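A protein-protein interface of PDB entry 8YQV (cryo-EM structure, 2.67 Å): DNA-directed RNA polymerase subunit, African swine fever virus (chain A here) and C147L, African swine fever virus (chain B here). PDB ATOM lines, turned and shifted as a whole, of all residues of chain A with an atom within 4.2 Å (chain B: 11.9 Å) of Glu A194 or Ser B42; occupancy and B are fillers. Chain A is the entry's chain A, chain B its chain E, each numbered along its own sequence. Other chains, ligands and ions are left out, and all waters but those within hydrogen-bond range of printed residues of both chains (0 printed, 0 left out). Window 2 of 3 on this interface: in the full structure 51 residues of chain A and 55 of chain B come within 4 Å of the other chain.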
ATOM      1  N   ASN A  19      14.877  10.345 -27.119  1.00  0.00           N
ATOM      2  CA  ASN A  19      14.585  10.925 -28.426  1.00  0.00           C
ATOM      3  C   ASN A  19      13.658  10.039 -29.242  1.00  0.00           C
ATOM      4  O   ASN A  19      12.786  10.546 -29.958  1.00  0.00           O
ATOM      5  CB  ASN A  19      15.880  11.175 -29.193  1.00  0.00           C
ATOM      6  CG  ASN A  19      16.957  11.780 -28.325  1.00  0.00           C
ATOM      7  OD1 ASN A  19      17.140  11.379 -27.178  1.00  0.00           O
ATOM      8  ND2 ASN A  19      17.676  12.756 -28.866  1.00  0.00           N
ATOM      9  N   ARG A 171      22.313   9.372 -15.047  1.00  0.00           N
ATOM     10  CA  ARG A 171      22.333  10.006 -16.361  1.00  0.00           C
ATOM     11  C   ARG A 171      23.478  10.999 -16.472  1.00  0.00           C
ATOM     12  O   ARG A 171      24.133  11.080 -17.516  1.00  0.00           O
ATOM     13  CB  ARG A 171      21.005  10.706 -16.658  1.00  0.00           C
ATOM     14  CG  ARG A 171      21.180  11.925 -17.569  1.00  0.00           C
ATOM     15  CD  ARG A 171      19.885  12.503 -18.118  1.00  0.00           C
ATOM     16  NE  ARG A 171      19.625  12.042 -19.476  1.00  0.00           N
ATOM     17  CZ  ARG A 171      18.763  11.089 -19.798  1.00  0.00           C
ATOM     18  NH1 ARG A 171      17.992  10.522 -18.889  1.00  0.00           N
ATOM     19  NH2 ARG A 171      18.660  10.707 -21.067  1.00  0.00           N
ATOM     20  N   PHE A 174      26.639   8.975 -16.994  1.00  0.00           N
ATOM     21  CA  PHE A 174      26.702   8.341 -18.304  1.00  0.00           C
ATOM     22  C   PHE A 174      26.812   9.346 -19.439  1.00  0.00           C
ATOM     23  O   PHE A 174      27.260   8.981 -20.529  1.00  0.00           O
ATOM     24  CB  PHE A 174      25.473   7.460 -18.519  1.00  0.00           C
ATOM     25  CG  PHE A 174      25.499   6.184 -17.736  1.00  0.00           C
ATOM     26  CD1 PHE A 174      26.658   5.762 -17.116  1.00  0.00           C
ATOM     27  CD2 PHE A 174      24.370   5.401 -17.631  1.00  0.00           C
ATOM     28  CE1 PHE A 174      26.687   4.589 -16.401  1.00  0.00           C
ATOM     29  CE2 PHE A 174      24.395   4.226 -16.920  1.00  0.00           C
ATOM     30  CZ  PHE A 174      25.555   3.822 -16.301  1.00  0.00           C
ATOM     31  N   TYR A 179      31.917   8.432 -27.105  1.00  0.00           N
ATOM     32  CA  TYR A 179      31.486   7.372 -28.009  1.00  0.00           C
ATOM     33  C   TYR A 179      32.600   6.379 -28.298  1.00  0.00           C
ATOM     34  O   TYR A 179      32.325   5.190 -28.489  1.00  0.00           O
ATOM     35  CB  TYR A 179      30.958   7.958 -29.316  1.00  0.00           C
ATOM     36  CG  TYR A 179      29.513   8.382 -29.245  1.00  0.00           C
ATOM     37  CD1 TYR A 179      28.493   7.444 -29.318  1.00  0.00           C
ATOM     38  CD2 TYR A 179      29.165   9.717 -29.116  1.00  0.00           C
ATOM     39  CE1 TYR A 179      27.169   7.825 -29.256  1.00  0.00           C
ATOM     40  CE2 TYR A 179      27.844  10.106 -29.053  1.00  0.00           C
ATOM     41  CZ  TYR A 179      26.851   9.156 -29.125  1.00  0.00           C
ATOM     42  OH  TYR A 179      25.533   9.541 -29.064  1.00  0.00           O
ATOM     43  N   HIS A 192      24.713   3.489 -26.491  1.00  0.00           N
ATOM     44  CA  HIS A 192      25.339   4.409 -25.557  1.00  0.00           C
ATOM     45  C   HIS A 192      24.645   4.313 -24.201  1.00  0.00           C
ATOM     46  O   HIS A 192      23.413   4.254 -24.141  1.00  0.00           O
ATOM     47  CB  HIS A 192      25.261   5.841 -26.089  1.00  0.00           C
ATOM     48  CG  HIS A 192      26.186   6.793 -25.401  1.00  0.00           C
ATOM     49  ND1 HIS A 192      25.914   7.327 -24.162  1.00  0.00           N
ATOM     50  CD2 HIS A 192      27.379   7.306 -25.778  1.00  0.00           C
ATOM     51  CE1 HIS A 192      26.901   8.125 -23.802  1.00  0.00           C
ATOM     52  NE2 HIS A 192      27.803   8.132 -24.767  1.00  0.00           N
ATOM     53  N   PRO A 193      25.399   4.282 -23.099  1.00  0.00           N
ATOM     54  CA  PRO A 193      24.779   4.032 -21.789  1.00  0.00           C
ATOM     55  C   PRO A 193      23.753   5.071 -21.371  1.00  0.00           C
ATOM     56  O   PRO A 193      22.861   4.739 -20.582  1.00  0.00           O
ATOM     57  CB  PRO A 193      25.976   4.019 -20.830  1.00  0.00           C
ATOM     58  CG  PRO A 193      27.053   4.740 -21.549  1.00  0.00           C
ATOM     59  CD  PRO A 193      26.856   4.429 -22.997  1.00  0.00           C
ATOM     60  N   GLU A 194      23.836   6.303 -21.876  1.00  0.00           N
ATOM     61  CA  GLU A 194      22.889   7.333 -21.468  1.00  0.00           C
ATOM     62  C   GLU A 194      21.452   6.969 -21.810  1.00  0.00           C
ATOM     63  O   GLU A 194      20.529   7.466 -21.158  1.00  0.00           O
ATOM     64  CB  GLU A 194      23.246   8.668 -22.117  1.00  0.00           C
ATOM     65  CG  GLU A 194      22.906   8.742 -23.588  1.00  0.00           C
ATOM     66  CD  GLU A 194      23.216  10.093 -24.184  1.00  0.00           C
ATOM     67  OE1 GLU A 194      23.691  10.976 -23.440  1.00  0.00           O
ATOM     68  OE2 GLU A 194      22.987  10.273 -25.396  1.00  0.00           O
ATOM     69  N   LYS A 195      21.242   6.103 -22.802  1.00  0.00           N
ATOM     70  CA  LYS A 195      19.900   5.683 -23.173  1.00  0.00           C
ATOM     71  C   LYS A 195      19.260   4.805 -22.114  1.00  0.00           C
ATOM     72  O   LYS A 195      18.075   4.479 -22.235  1.00  0.00           O
ATOM     73  CB  LYS A 195      19.935   4.945 -24.508  1.00  0.00           C
ATOM     74  CG  LYS A 195      20.571   5.755 -25.614  1.00  0.00           C
ATOM     75  CD  LYS A 195      20.656   4.982 -26.911  1.00  0.00           C
ATOM     76  CE  LYS A 195      19.328   4.983 -27.629  1.00  0.00           C
ATOM     77  NZ  LYS A 195      19.481   4.591 -29.053  1.00  0.00           N
ATOM     78  N   LEU A 196      20.014   4.409 -21.095  1.00  0.00           N
ATOM     79  CA  LEU A 196      19.499   3.528 -20.062  1.00  0.00           C
ATOM     80  C   LEU A 196      18.714   4.260 -18.982  1.00  0.00           C
ATOM     81  O   LEU A 196      18.124   3.602 -18.119  1.00  0.00           O
ATOM     82  CB  LEU A 196      20.656   2.754 -19.435  1.00  0.00           C
ATOM     83  CG  LEU A 196      21.448   1.872 -20.396  1.00  0.00           C
ATOM     84  CD1 LEU A 196      22.667   1.308 -19.709  1.00  0.00           C
ATOM     85  CD2 LEU A 196      20.568   0.766 -20.910  1.00  0.00           C
ATOM     86  N   VAL A 197      18.687   5.590 -19.000  1.00  0.00           N
ATOM     87  CA  VAL A 197      17.941   6.377 -18.028  1.00  0.00           C
ATOM     88  C   VAL A 197      16.945   7.230 -18.800  1.00  0.00           C
ATOM     89  O   VAL A 197      17.318   7.901 -19.767  1.00  0.00           O
ATOM     90  CB  VAL A 197      18.872   7.248 -17.161  1.00  0.00           C
ATOM     91  CG1 VAL A 197      18.134   8.447 -16.614  1.00  0.00           C
ATOM     92  CG2 VAL A 197      19.484   6.434 -16.042  1.00  0.00           C
ATOM     93  N   SER B  42      21.875   9.683 -27.748  1.00  0.00           N
ATOM     94  CA  SER B  42      21.613  11.067 -28.139  1.00  0.00           C
ATOM     95  C   SER B  42      20.744  11.180 -29.401  1.00  0.00           C
ATOM     96  O   SER B  42      19.796  11.962 -29.411  1.00  0.00           O
ATOM     97  CB  SER B  42      22.933  11.809 -28.359  1.00  0.00           C
ATOM     98  OG  SER B  42      23.650  11.262 -29.452  1.00  0.00           O
ATOM     99  N   PRO B  43      21.047  10.419 -30.473  1.00  0.00           N
ATOM    100  CA  PRO B  43      20.138  10.424 -31.624  1.00  0.00           C
ATOM    101  C   PRO B  43      19.051   9.366 -31.518  1.00  0.00           C
ATOM    102  O   PRO B  43      18.953   8.656 -30.513  1.00  0.00           O
ATOM    103  CB  PRO B  43      21.076  10.141 -32.799  1.00  0.00           C
ATOM    104  CG  PRO B  43      22.076   9.224 -32.216  1.00  0.00           C
ATOM    105  CD  PRO B  43      22.286   9.678 -30.791  1.00  0.00           C
ATOM    106  N   SER B  44      18.223   9.265 -32.550  1.00  0.00           N
ATOM    107  CA  SER B  44      17.271   8.176 -32.676  1.00  0.00           C
ATOM    108  C   SER B  44      17.886   7.051 -33.510  1.00  0.00           C
ATOM    109  O   SER B  44      18.862   7.247 -34.236  1.00  0.00           O
ATOM    110  CB  SER B  44      15.969   8.681 -33.305  1.00  0.00           C
ATOM    111  OG  SER B  44      14.975   7.672 -33.344  1.00  0.00           O
ATOM    112  N   ILE B  45      17.313   5.852 -33.389  1.00  0.00           N
ATOM    113  CA  ILE B  45      17.794   4.742 -34.208  1.00  0.00           C
ATOM    114  C   ILE B  45      17.574   5.033 -35.687  1.00  0.00           C
ATOM    115  O   ILE B  45      18.408   4.671 -36.528  1.00  0.00           O
ATOM    116  CB  ILE B  45      17.135   3.414 -33.782  1.00  0.00           C
ATOM    117  CG1 ILE B  45      17.768   2.879 -32.496  1.00  0.00           C
ATOM    118  CG2 ILE B  45      17.245   2.370 -34.879  1.00  0.00           C
ATOM    119  CD1 ILE B  45      17.165   3.393 -31.229  1.00  0.00           C
ATOM    120  N   CYS B  46      16.478   5.711 -36.033  1.00  0.00           N
ATOM    121  CA  CYS B  46      16.197   6.031 -37.427  1.00  0.00           C
ATOM    122  C   CYS B  46      17.242   6.946 -38.049  1.00  0.00           C
ATOM    123  O   CYS B  46      17.302   7.036 -39.280  1.00  0.00           O
ATOM    124  CB  CYS B  46      14.817   6.677 -37.553  1.00  0.00           C
ATOM    125  SG  CYS B  46      14.712   8.375 -36.950  1.00  0.00           S
ATOM    126  N   GLU B  47      18.055   7.627 -37.240  1.00  0.00           N
ATOM    127  CA  GLU B  47      19.094   8.512 -37.753  1.00  0.00           C
ATOM    128  C   GLU B  47      20.125   7.733 -38.556  1.00  0.00           C
ATOM    129  O   GLU B  47      20.317   7.989 -39.750  1.00  0.00           O
ATOM    130  CB  GLU B  47      19.782   9.258 -36.608  1.00  0.00           C
ATOM    131  CG  GLU B  47      20.834  10.266 -37.061  1.00  0.00           C
ATOM    132  CD  GLU B  47      22.226   9.671 -37.136  1.00  0.00           C
ATOM    133  OE1 GLU B  47      22.516   8.740 -36.358  1.00  0.00           O
ATOM    134  OE2 GLU B  47      23.026  10.128 -37.978  1.00  0.00           O
ATOM    135  N   GLY B  48      20.796   6.791 -37.905  1.00  0.00           N
ATOM    136  CA  GLY B  48      21.796   5.982 -38.563  1.00  0.00           C
ATOM    137  C   GLY B  48      21.253   4.886 -39.440  1.00  0.00           C
ATOM    138  O   GLY B  48      22.029   4.213 -40.124  1.00  0.00           O
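The side-chain hydroxyl of Tyr A179 lies within hydrogen-bond range of the side-chain hydroxyl of Ser B42, 2.6 Å away. N of Ser B42 sits at hydrogen-bond distance from OE2 of Glu A194, at 2.7 Å. O of Ser B42 sits close to ND2 of Asn A19, at 2.3 Å.
A ring nitrogen (ND1) of His A192 sits close to the backbone NH (N) of Glu A194 (3.3 Å).
Among the printed residues, merely in contact across the chains: Lys A195 with Ile B45 (3.4 Å) and Tyr A179 with Pro B43 (3.7 Å).
Of chain B, only Ser B42 (2.3 Å) comes within 4 Å of Asn A19. Of the printed residues of chain B, Tyr A179 touches Ser B42 (2.6 Å) and Pro B43 (3.7 Å). No residue of chain B comes within 4 Å of His A192. No residue of chain B comes within 4 Å of Pro A193. Of chain B, only Ser B42 comes within 4 Å of Glu A194. Lys A195 touches just one residue of chain B: Ile B45 (3.4 Å). No residue of chain B comes within 4 Å of Val A197. Of chain A, only Asn A19 (2.3 Å), Tyr A179 (2.6 Å) and Glu A194 (2.7 Å) come within 4 Å of Ser B42. Of the printed residues of chain A, Pro B43 touches Tyr A179. Printed residues of chain A within 4 Å of Ile B45: Lys A195 (3.4 Å). The nearest residue of chain B that does not touch Glu A194 is Pro B43 (5.4 Å). The nearest printed residue of chain A that does not touch Ile B45 is Asn A19 (6.9 Å).
Of the 7 printed residues of chain B, 3 touch a printed residue of chain A. Printed residues of chain B that touch a printed residue of chain A: Ser B42, Pro B43 and Ile B45. Along chain B the printed residues that touch a printed residue of chain A span positions 42 to 45. Hydrophobic or aromatic side chains of chain A within 4 Å of the printed part of chain B: Tyr A179. Along chain A the printed residues that touch a printed residue of chain B span positions 19 to 195. Among the printed residues, 5 pairs touch across the chains. Among the printed residues, no Asp or Glu carboxylate lies within 4 Å of a Lys or Arg side-chain nitrogen of the other chain.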
